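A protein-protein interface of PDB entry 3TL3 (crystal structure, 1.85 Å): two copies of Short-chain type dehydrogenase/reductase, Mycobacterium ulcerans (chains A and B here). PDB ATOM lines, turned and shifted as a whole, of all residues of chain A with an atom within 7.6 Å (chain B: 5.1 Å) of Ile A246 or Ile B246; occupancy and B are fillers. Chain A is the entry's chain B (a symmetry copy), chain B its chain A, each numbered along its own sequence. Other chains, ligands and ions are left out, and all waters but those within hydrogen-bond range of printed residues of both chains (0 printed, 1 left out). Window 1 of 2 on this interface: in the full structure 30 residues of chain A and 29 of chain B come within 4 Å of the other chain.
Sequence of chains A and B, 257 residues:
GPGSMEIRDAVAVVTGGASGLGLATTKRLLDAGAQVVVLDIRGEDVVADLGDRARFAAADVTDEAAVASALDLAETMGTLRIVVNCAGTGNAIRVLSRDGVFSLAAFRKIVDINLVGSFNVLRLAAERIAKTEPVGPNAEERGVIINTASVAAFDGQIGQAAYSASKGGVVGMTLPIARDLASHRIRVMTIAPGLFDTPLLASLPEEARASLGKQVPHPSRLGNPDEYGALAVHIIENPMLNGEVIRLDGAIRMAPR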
ATOM      1  N   ASN A 147       8.821   7.376 -19.870  1.00  0.00           N
ATOM      2  CA  ASN A 147       9.590   7.826 -21.035  1.00  0.00           C
ATOM      3  C   ASN A 147       9.918   9.298 -20.939  1.00  0.00           C
ATOM      4  O   ASN A 147       9.286  10.013 -20.192  1.00  0.00           O
ATOM      5  CB  ASN A 147       8.806   7.595 -22.317  1.00  0.00           C
ATOM      6  CG  ASN A 147       8.270   6.204 -22.413  1.00  0.00           C
ATOM      7  OD1 ASN A 147       9.040   5.250 -22.382  1.00  0.00           O
ATOM      8  ND2 ASN A 147       6.944   6.063 -22.473  1.00  0.00           N
ATOM      9  N   ALA A 149      10.246  12.530 -23.506  1.00  0.00           N
ATOM     10  CA  ALA A 149      10.003  13.117 -24.819  1.00  0.00           C
ATOM     11  C   ALA A 149      10.795  14.418 -24.925  1.00  0.00           C
ATOM     12  O   ALA A 149      10.369  15.433 -24.397  1.00  0.00           O
ATOM     13  CB  ALA A 149       8.497  13.383 -24.999  1.00  0.00           C
ATOM     14  N   VAL A 171       5.613  10.651 -27.497  1.00  0.00           N
ATOM     15  CA  VAL A 171       4.290  11.123 -27.109  1.00  0.00           C
ATOM     16  C   VAL A 171       3.195  10.238 -27.707  1.00  0.00           C
ATOM     17  O   VAL A 171       2.287   9.822 -27.000  1.00  0.00           O
ATOM     18  CB  VAL A 171       4.062  12.582 -27.541  1.00  0.00           C
ATOM     19  CG1 VAL A 171       2.570  12.951 -27.456  1.00  0.00           C
ATOM     20  CG2 VAL A 171       4.926  13.521 -26.696  1.00  0.00           C
ATOM     21  N   THR A 174       2.468   6.783 -26.083  1.00  0.00           N
ATOM     22  CA  THR A 174       2.283   6.712 -24.634  1.00  0.00           C
ATOM     23  C   THR A 174       0.925   6.147 -24.243  1.00  0.00           C
ATOM     24  O   THR A 174       0.842   5.164 -23.478  1.00  0.00           O
ATOM     25  CB  THR A 174       2.531   8.081 -23.983  1.00  0.00           C
ATOM     26  OG1 THR A 174       3.892   8.464 -24.204  1.00  0.00           O
ATOM     27  CG2 THR A 174       2.244   8.031 -22.477  1.00  0.00           C
ATOM     28  N   MET A 189       3.941   6.240 -18.625  1.00  0.00           N
ATOM     29  CA  MET A 189       3.870   7.702 -18.558  1.00  0.00           C
ATOM     30  C   MET A 189       5.048   8.320 -19.293  1.00  0.00           C
ATOM     31  O   MET A 189       6.077   7.658 -19.501  1.00  0.00           O
ATOM     32  CB  MET A 189       3.933   8.181 -17.103  1.00  0.00           C
ATOM     33  CG  MET A 189       2.667   7.961 -16.293  1.00  0.00           C
ATOM     34  SD  MET A 189       1.311   9.059 -16.759  1.00  0.00           S
ATOM     35  CE  MET A 189       2.026  10.677 -16.401  1.00  0.00           C
ATOM     36  N   THR A 190       4.915   9.607 -19.627  1.00  0.00           N
ATOM     37  CA  THR A 190       5.977  10.323 -20.319  1.00  0.00           C
ATOM     38  C   THR A 190       6.185  11.721 -19.726  1.00  0.00           C
ATOM     39  O   THR A 190       5.223  12.432 -19.432  1.00  0.00           O
ATOM     40  CB  THR A 190       5.651  10.396 -21.825  1.00  0.00           C
ATOM     41  OG1 THR A 190       5.708   9.086 -22.385  1.00  0.00           O
ATOM     42  CG2 THR A 190       6.603  11.312 -22.604  1.00  0.00           C
ATOM     43  N   ILE A 191       7.444  12.098 -19.535  1.00  0.00           N
ATOM     44  CA  ILE A 191       7.766  13.467 -19.155  1.00  0.00           C
ATOM     45  C   ILE A 191       8.344  14.136 -20.389  1.00  0.00           C
ATOM     46  O   ILE A 191       9.210  13.573 -21.066  1.00  0.00           O
ATOM     47  CB  ILE A 191       8.776  13.535 -17.979  1.00  0.00           C
ATOM     48  CG1 ILE A 191       8.210  12.848 -16.726  1.00  0.00           C
ATOM     49  CG2 ILE A 191       9.135  15.003 -17.684  1.00  0.00           C
ATOM     50  CD1 ILE A 191       9.281  12.522 -15.672  1.00  0.00           C
ATOM     51  N   ALA A 192       7.845  15.334 -20.684  1.00  0.00           N
ATOM     52  CA  ALA A 192       8.348  16.159 -21.773  1.00  0.00           C
ATOM     53  C   ALA A 192       9.090  17.379 -21.225  1.00  0.00           C
ATOM     54  O   ALA A 192       8.473  18.425 -20.977  1.00  0.00           O
ATOM     55  CB  ALA A 192       7.182  16.593 -22.651  1.00  0.00           C
ATOM     56  N   PRO A 193      10.411  17.244 -21.010  1.00  0.00           N
ATOM     57  CA  PRO A 193      11.111  18.372 -20.410  1.00  0.00           C
ATOM     58  C   PRO A 193      11.352  19.506 -21.390  1.00  0.00           C
ATOM     59  O   PRO A 193      11.446  19.298 -22.615  1.00  0.00           O
ATOM     60  CB  PRO A 193      12.441  17.774 -19.931  1.00  0.00           C
ATOM     61  CG  PRO A 193      12.603  16.492 -20.651  1.00  0.00           C
ATOM     62  CD  PRO A 193      11.301  16.099 -21.276  1.00  0.00           C
ATOM     63  N   GLY A 194      11.430  20.715 -20.841  1.00  0.00           N
ATOM     64  CA  GLY A 194      11.924  21.865 -21.608  1.00  0.00           C
ATOM     65  C   GLY A 194      13.430  21.928 -21.486  1.00  0.00           C
ATOM     66  O   GLY A 194      14.105  20.906 -21.575  1.00  0.00           O
ATOM     67  N   TYR A 228      13.330  17.105 -12.632  1.00  0.00           N
ATOM     68  CA  TYR A 228      12.868  15.978 -13.430  1.00  0.00           C
ATOM     69  C   TYR A 228      12.765  14.721 -12.552  1.00  0.00           C
ATOM     70  O   TYR A 228      11.783  13.985 -12.621  1.00  0.00           O
ATOM     71  CB  TYR A 228      13.826  15.715 -14.589  1.00  0.00           C
ATOM     72  CG  TYR A 228      13.463  14.504 -15.396  1.00  0.00           C
ATOM     73  CD1 TYR A 228      12.798  14.628 -16.605  1.00  0.00           C
ATOM     74  CD2 TYR A 228      13.765  13.209 -14.930  1.00  0.00           C
ATOM     75  CE1 TYR A 228      12.460  13.516 -17.351  1.00  0.00           C
ATOM     76  CE2 TYR A 228      13.421  12.088 -15.665  1.00  0.00           C
ATOM     77  CZ  TYR A 228      12.761  12.239 -16.870  1.00  0.00           C
ATOM     78  OH  TYR A 228      12.370  11.142 -17.608  1.00  0.00           O
ATOM     79  N   LEU A 231       9.756  14.686 -10.268  1.00  0.00           N
ATOM     80  CA  LEU A 231       8.529  14.354 -10.980  1.00  0.00           C
ATOM     81  C   LEU A 231       8.444  12.842 -11.260  1.00  0.00           C
ATOM     82  O   LEU A 231       7.370  12.231 -11.125  1.00  0.00           O
ATOM     83  CB  LEU A 231       8.444  15.141 -12.299  1.00  0.00           C
ATOM     84  CG  LEU A 231       7.198  14.865 -13.149  1.00  0.00           C
ATOM     85  CD1 LEU A 231       5.874  15.018 -12.394  1.00  0.00           C
ATOM     86  CD2 LEU A 231       7.228  15.778 -14.359  1.00  0.00           C
ATOM     87  N   HIS A 234       7.378  11.179  -8.215  1.00  0.00           N
ATOM     88  CA  HIS A 234       5.965  11.416  -7.966  1.00  0.00           C
ATOM     89  C   HIS A 234       5.088  10.527  -8.834  1.00  0.00           C
ATOM     90  O   HIS A 234       4.126   9.945  -8.342  1.00  0.00           O
ATOM     91  CB  HIS A 234       5.538  12.873  -8.144  1.00  0.00           C
ATOM     92  CG  HIS A 234       4.100  13.049  -7.801  1.00  0.00           C
ATOM     93  ND1 HIS A 234       3.653  12.854  -6.558  1.00  0.00           N
ATOM     94  CD2 HIS A 234       2.971  13.224  -8.608  1.00  0.00           C
ATOM     95  CE1 HIS A 234       2.306  12.994  -6.547  1.00  0.00           C
ATOM     96  NE2 HIS A 234       1.896  13.198  -7.808  1.00  0.00           N
ATOM     97  N   ILE A 235       5.441  10.385 -10.114  1.00  0.00           N
ATOM     98  CA  ILE A 235       4.694   9.540 -11.019  1.00  0.00           C
ATOM     99  C   ILE A 235       4.674   8.094 -10.499  1.00  0.00           C
ATOM    100  O   ILE A 235       3.627   7.434 -10.474  1.00  0.00           O
ATOM    101  CB  ILE A 235       5.298   9.589 -12.455  1.00  0.00           C
ATOM    102  CG1 ILE A 235       5.017  10.935 -13.101  1.00  0.00           C
ATOM    103  CG2 ILE A 235       4.726   8.476 -13.334  1.00  0.00           C
ATOM    104  CD1 ILE A 235       5.768  11.173 -14.408  1.00  0.00           C
ATOM    105  N   LEU A 241      -1.752   8.190 -12.154  1.00  0.00           N
ATOM    106  CA  LEU A 241      -1.126   8.794 -13.323  1.00  0.00           C
ATOM    107  C   LEU A 241      -0.796   7.702 -14.346  1.00  0.00           C
ATOM    108  O   LEU A 241       0.149   6.925 -14.187  1.00  0.00           O
ATOM    109  CB  LEU A 241       0.137   9.584 -12.943  1.00  0.00           C
ATOM    110  CG  LEU A 241      -0.073  10.949 -12.265  1.00  0.00           C
ATOM    111  CD1 LEU A 241       1.218  11.508 -11.662  1.00  0.00           C
ATOM    112  CD2 LEU A 241      -0.657  11.980 -13.221  1.00  0.00           C
ATOM    113  N   GLU A 244      -0.324   9.359 -19.825  1.00  0.00           N
ATOM    114  CA  GLU A 244      -0.279  10.811 -19.944  1.00  0.00           C
ATOM    115  C   GLU A 244       1.136  11.328 -20.206  1.00  0.00           C
ATOM    116  O   GLU A 244       2.111  10.720 -19.799  1.00  0.00           O
ATOM    117  CB  GLU A 244      -0.873  11.443 -18.666  1.00  0.00           C
ATOM    118  CG  GLU A 244      -0.626  12.917 -18.447  1.00  0.00           C
ATOM    119  CD  GLU A 244      -1.303  13.841 -19.451  1.00  0.00           C
ATOM    120  OE1 GLU A 244      -1.480  13.497 -20.632  1.00  0.00           O
ATOM    121  OE2 GLU A 244      -1.641  14.978 -19.081  1.00  0.00           O
ATOM    122  N   VAL A 245       1.213  12.452 -20.908  1.00  0.00           N
ATOM    123  CA  VAL A 245       2.462  13.192 -21.091  1.00  0.00           C
ATOM    124  C   VAL A 245       2.415  14.406 -20.166  1.00  0.00           C
ATOM    125  O   VAL A 245       1.456  15.164 -20.213  1.00  0.00           O
ATOM    126  CB  VAL A 245       2.617  13.668 -22.552  1.00  0.00           C
ATOM    127  CG1 VAL A 245       3.881  14.534 -22.729  1.00  0.00           C
ATOM    128  CG2 VAL A 245       2.631  12.481 -23.510  1.00  0.00           C
ATOM    129  N   ILE A 246       3.457  14.619 -19.367  1.00  0.00           N
ATOM    130  CA  ILE A 246       3.538  15.820 -18.516  1.00  0.00           C
ATOM    131  C   ILE A 246       4.654  16.717 -18.985  1.00  0.00           C
ATOM    132  O   ILE A 246       5.820  16.347 -18.912  1.00  0.00           O
ATOM    133  CB  ILE A 246       3.787  15.455 -17.036  1.00  0.00           C
ATOM    134  CG1 ILE A 246       2.688  14.506 -16.546  1.00  0.00           C
ATOM    135  CG2 ILE A 246       3.851  16.732 -16.174  1.00  0.00           C
ATOM    136  CD1 ILE A 246       2.816  14.073 -15.099  1.00  0.00           C
ATOM    137  N   ARG A 247       4.299  17.899 -19.471  1.00  0.00           N
ATOM    138  CA  ARG A 247       5.301  18.884 -19.834  1.00  0.00           C
ATOM    139  C   ARG A 247       5.928  19.464 -18.563  1.00  0.00           C
ATOM    140  O   ARG A 247       5.208  19.857 -17.653  1.00  0.00           O
ATOM    141  CB  ARG A 247       4.650  19.990 -20.646  1.00  0.00           C
ATOM    142  CG  ARG A 247       4.047  19.520 -21.963  1.00  0.00           C
ATOM    143  CD  ARG A 247       3.358  20.689 -22.636  1.00  0.00           C
ATOM    144  NE  ARG A 247       4.376  21.642 -23.074  1.00  0.00           N
ATOM    145  CZ  ARG A 247       4.669  21.945 -24.342  1.00  0.00           C
ATOM    146  NH1 ARG A 247       3.976  21.447 -25.367  1.00  0.00           N
ATOM    147  NH2 ARG A 247       5.654  22.805 -24.583  1.00  0.00           N
ATOM    148  N   LEU A 248       7.248  19.548 -18.534  1.00  0.00           N
ATOM    149  CA  LEU A 248       8.004  20.072 -17.388  1.00  0.00           C
ATOM    150  C   LEU A 248       8.950  21.124 -17.951  1.00  0.00           C
ATOM    151  O   LEU A 248      10.109  20.839 -18.272  1.00  0.00           O
ATOM    152  CB  LEU A 248       8.767  18.951 -16.689  1.00  0.00           C
ATOM    153  CG  LEU A 248       9.624  19.274 -15.472  1.00  0.00           C
ATOM    154  CD1 LEU A 248       8.731  19.732 -14.317  1.00  0.00           C
ATOM    155  CD2 LEU A 248      10.469  18.062 -15.060  1.00  0.00           C
ATOM    156  N   ASP A 249       8.435  22.335 -18.128  1.00  0.00           N
ATOM    157  CA  ASP A 249       9.127  23.279 -18.991  1.00  0.00           C
ATOM    158  C   ASP A 249       8.944  24.760 -18.730  1.00  0.00           C
ATOM    159  O   ASP A 249       9.272  25.581 -19.598  1.00  0.00           O
ATOM    160  CB  ASP A 249       8.725  22.975 -20.429  1.00  0.00           C
ATOM    161  CG  ASP A 249       7.247  23.259 -20.704  1.00  0.00           C
ATOM    162  OD1 ASP A 249       6.584  23.948 -19.898  1.00  0.00           O
ATOM    163  OD2 ASP A 249       6.748  22.758 -21.741  1.00  0.00           O
ATOM    164  N   MET B 189      -1.261  26.077 -13.287  1.00  0.00           N
ATOM    165  CA  MET B 189      -1.322  24.663 -13.688  1.00  0.00           C
ATOM    166  C   MET B 189      -2.736  24.162 -13.582  1.00  0.00           C
ATOM    167  O   MET B 189      -3.555  24.749 -12.895  1.00  0.00           O
ATOM    168  CB  MET B 189      -0.462  23.808 -12.777  1.00  0.00           C
ATOM    169  CG  MET B 189       1.037  23.970 -12.985  1.00  0.00           C
ATOM    170  SD  MET B 189       1.638  23.191 -14.469  1.00  0.00           S
ATOM    171  CE  MET B 189       1.119  21.488 -14.183  1.00  0.00           C
ATOM    172  N   THR B 190      -3.021  23.076 -14.295  1.00  0.00           N
ATOM    173  CA  THR B 190      -4.348  22.474 -14.268  1.00  0.00           C
ATOM    174  C   THR B 190      -4.230  20.987 -14.096  1.00  0.00           C
ATOM    175  O   THR B 190      -3.400  20.351 -14.741  1.00  0.00           O
ATOM    176  CB  THR B 190      -5.134  22.790 -15.549  1.00  0.00           C
ATOM    177  OG1 THR B 190      -5.434  24.191 -15.586  1.00  0.00           O
ATOM    178  CG2 THR B 190      -6.429  21.981 -15.626  1.00  0.00           C
ATOM    179  N   ILE B 191      -5.059  20.438 -13.223  1.00  0.00           N
ATOM    180  CA  ILE B 191      -5.218  18.999 -13.100  1.00  0.00           C
ATOM    181  C   ILE B 191      -6.559  18.617 -13.725  1.00  0.00           C
ATOM    182  O   ILE B 191      -7.584  19.260 -13.454  1.00  0.00           O
ATOM    183  CB  ILE B 191      -5.235  18.531 -11.642  1.00  0.00           C
ATOM    184  CG1 ILE B 191      -3.883  18.759 -10.951  1.00  0.00           C
ATOM    185  CG2 ILE B 191      -5.537  17.020 -11.603  1.00  0.00           C
ATOM    186  CD1 ILE B 191      -3.911  18.686  -9.427  1.00  0.00           C
ATOM    187  N   ALA B 192      -6.548  17.586 -14.559  1.00  0.00           N
ATOM    188  CA  ALA B 192      -7.755  17.100 -15.238  1.00  0.00           C
ATOM    189  C   ALA B 192      -8.064  15.703 -14.721  1.00  0.00           C
ATOM    190  O   ALA B 192      -7.530  14.709 -15.234  1.00  0.00           O
ATOM    191  CB  ALA B 192      -7.537  17.070 -16.757  1.00  0.00           C
ATOM    192  N   LEU B 231      -0.838  15.042  -6.044  1.00  0.00           N
ATOM    193  CA  LEU B 231      -0.391  15.713  -7.268  1.00  0.00           C
ATOM    194  C   LEU B 231      -0.363  17.234  -7.095  1.00  0.00           C
ATOM    195  O   LEU B 231       0.586  17.910  -7.543  1.00  0.00           O
ATOM    196  CB  LEU B 231      -1.313  15.369  -8.464  1.00  0.00           C
ATOM    197  CG  LEU B 231      -0.976  16.012  -9.822  1.00  0.00           C
ATOM    198  CD1 LEU B 231       0.482  15.760 -10.201  1.00  0.00           C
ATOM    199  CD2 LEU B 231      -1.903  15.517 -10.938  1.00  0.00           C
ATOM    200  N   ILE B 235       2.895  19.598  -7.555  1.00  0.00           N
ATOM    201  CA  ILE B 235       2.933  20.752  -8.465  1.00  0.00           C
ATOM    202  C   ILE B 235       3.472  21.967  -7.705  1.00  0.00           C
ATOM    203  O   ILE B 235       4.338  22.722  -8.197  1.00  0.00           O
ATOM    204  CB  ILE B 235       1.532  21.060  -9.060  1.00  0.00           C
ATOM    205  CG1 ILE B 235       1.108  19.973 -10.069  1.00  0.00           C
ATOM    206  CG2 ILE B 235       1.534  22.452  -9.723  1.00  0.00           C
ATOM    207  CD1 ILE B 235      -0.392  19.996 -10.422  1.00  0.00           C
ATOM    208  N   LEU B 241       7.045  22.982 -13.117  1.00  0.00           N
ATOM    209  CA  LEU B 241       5.716  22.712 -13.653  1.00  0.00           C
ATOM    210  C   LEU B 241       4.934  24.002 -13.824  1.00  0.00           C
ATOM    211  O   LEU B 241       4.482  24.599 -12.846  1.00  0.00           O
ATOM    212  CB  LEU B 241       4.962  21.760 -12.726  1.00  0.00           C
ATOM    213  CG  LEU B 241       5.508  20.348 -12.797  1.00  0.00           C
ATOM    214  CD1 LEU B 241       4.829  19.479 -11.748  1.00  0.00           C
ATOM    215  CD2 LEU B 241       5.318  19.743 -14.187  1.00  0.00           C
ATOM    216  N   GLU B 244       0.711  23.950 -17.800  1.00  0.00           N
ATOM    217  CA  GLU B 244       0.453  22.600 -18.265  1.00  0.00           C
ATOM    218  C   GLU B 244      -0.788  22.008 -17.629  1.00  0.00           C
ATOM    219  O   GLU B 244      -1.163  22.373 -16.525  1.00  0.00           O
ATOM    220  CB  GLU B 244       1.690  21.719 -17.991  1.00  0.00           C
ATOM    221  CG  GLU B 244       1.532  20.200 -18.119  1.00  0.00           C
ATOM    222  CD  GLU B 244       1.247  19.687 -19.525  1.00  0.00           C
ATOM    223  OE1 GLU B 244       0.591  20.368 -20.348  1.00  0.00           O
ATOM    224  OE2 GLU B 244       1.652  18.549 -19.814  1.00  0.00           O
ATOM    225  N   VAL B 245      -1.423  21.100 -18.362  1.00  0.00           N
ATOM    226  CA  VAL B 245      -2.553  20.323 -17.860  1.00  0.00           C
ATOM    227  C   VAL B 245      -2.051  18.914 -17.605  1.00  0.00           C
ATOM    228  O   VAL B 245      -1.399  18.339 -18.468  1.00  0.00           O
ATOM    229  CB  VAL B 245      -3.722  20.277 -18.855  1.00  0.00           C
ATOM    230  CG1 VAL B 245      -4.856  19.397 -18.291  1.00  0.00           C
ATOM    231  CG2 VAL B 245      -4.232  21.698 -19.127  1.00  0.00           C
ATOM    232  N   ILE B 246      -2.312  18.380 -16.419  1.00  0.00           N
ATOM    233  CA  ILE B 246      -1.935  16.999 -16.092  1.00  0.00           C
ATOM    234  C   ILE B 246      -3.193  16.151 -15.923  1.00  0.00           C
ATOM    235  O   ILE B 246      -3.962  16.333 -14.970  1.00  0.00           O
ATOM    236  CB  ILE B 246      -1.079  16.899 -14.807  1.00  0.00           C
ATOM    237  CG1 ILE B 246       0.185  17.767 -14.925  1.00  0.00           C
ATOM    238  CG2 ILE B 246      -0.718  15.429 -14.526  1.00  0.00           C
ATOM    239  CD1 ILE B 246       1.094  17.732 -13.717  1.00  0.00           C
ATOM    240  N   ARG B 247      -3.391  15.193 -16.836  1.00  0.00           N
ATOM    241  CA  ARG B 247      -4.502  14.269 -16.707  1.00  0.00           C
ATOM    242  C   ARG B 247      -4.183  13.258 -15.602  1.00  0.00           C
ATOM    243  O   ARG B 247      -3.072  12.696 -15.558  1.00  0.00           O
ATOM    244  CB  ARG B 247      -4.735  13.550 -18.053  1.00  0.00           C
ATOM    245  N   LEU B 248      -5.134  13.057 -14.696  1.00  0.00           N
ATOM    246  CA  LEU B 248      -4.987  12.132 -13.600  1.00  0.00           C
ATOM    247  C   LEU B 248      -6.178  11.203 -13.667  1.00  0.00           C
ATOM    248  O   LEU B 248      -7.223  11.489 -13.065  1.00  0.00           O
ATOM    249  CB  LEU B 248      -4.963  12.927 -12.276  1.00  0.00           C
ATOM    250  CG  LEU B 248      -4.766  12.138 -10.983  1.00  0.00           C
ATOM    251  CD1 LEU B 248      -3.354  11.544 -10.969  1.00  0.00           C
ATOM    252  CD2 LEU B 248      -4.995  13.058  -9.775  1.00  0.00           C
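The side-chain carboxylate of Glu A244 lies close to the backbone carbonyl oxygen of Val B245 (3.4 Å). The side-chain carboxylate (OE2) of Glu B244 sits close to the backbone carbonyl oxygen (O) of Val A245 (3.4 Å). The side-chain carboxylate of Glu A244 sits at hydrogen-bond distance from the backbone NH of Arg B247. The side-chain carboxylate (OE2) of Glu B244 sits at hydrogen-bond distance from the backbone NH (N) of Arg A247.
The backbone NH (N) of Ile A246 sits at hydrogen-bond distance from the backbone carbonyl oxygen (O) of Thr A190 (2.8 Å). N of Gly A194 is in hydrogen-bond range of O of Leu A248, at 2.9 Å. The backbone carbonyl oxygen (O) of Ala A192 is in hydrogen-bond range of the backbone NH (N) of Leu A248 (3.0 Å). The backbone carbonyl oxygen of Ala B192 is in hydrogen-bond range of the backbone NH of Leu B248, at 3.0 Å. The backbone carbonyl oxygen (O) of Glu B244 sits at hydrogen-bond distance from the backbone NH (N) of Thr B190 (3.0 Å). N of Ala A192 lies within hydrogen-bond range of O of Ile A246, at 2.9 Å.
Among the printed residues, pairs that only touch across the chains: Leu A248 with Leu B241 (3.4 Å), Leu A241 with Arg B247 (3.4 Å), His A234 with Leu B231 (3.4 Å), Arg A247 with Leu B241 (3.5 Å), Leu A241 with Leu B248 (3.5 Å), Ile A246 with Glu B244 (3.6 Å), Glu A244 with Ile B246 (3.6 Å), Leu A241 with Ile B246 (3.7 Å), Ile A246 with Ile B246 (3.8 Å) and Ile A246 with Leu B241 (3.9 Å).
Ile A246 touches just these residues of chain B: Leu B241, Glu B244 and Ile B246. Of chain A, only Leu A241 (3.7 Å), Glu A244 (3.6 Å) and Ile A246 (3.8 Å) come within 4 Å of Ile B246. Printed residues of chain A within 4 Å of Leu B231: His A234. Of the printed residues of chain B, Val A245 touches Glu B244. Printed residues of chain B within 4 Å of Glu A244: Val B245 (3.4 Å), Ile B246 (3.6 Å) and Arg B247 (2.9 Å). Printed residues of chain B within 4 Å of His A234: Leu B231 (3.4 Å). The nearest printed residue of chain B that does not touch Ile A246 is Val B245 (5.5 Å).
Hydrophobic or aromatic side chains of chain B within 4 Å of the printed part of chain A: Leu B231, Leu B241, Ile B246 and Leu B248. Among the printed residues, 14 pairs touch across the chains. Among the printed residues, no Asp or Glu carboxylate lies within 4 Å of a Lys or Arg side-chain nitrogen of the other chain.
Leu A241 touches Ile B246, and with the chains exchanged Ile A246 touches Leu B241. Leu A241 touches Leu B248, and with the chains exchanged Leu A248 touches Leu B241. Glu A244 touches Ile B246, and with the chains exchanged Ile A246 touches Glu B244. Glu A244 touches Arg B247, and with the chains exchanged Arg A247 touches Glu B244. Positions printed for both chains: 189, 190, 191, 192, 231, 235, 241, 244, 245, 246, 247 and 248. Of the 14 pairs that touch across the chains among the printed residues, 13 have their exchanged pair printed and touching as well.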
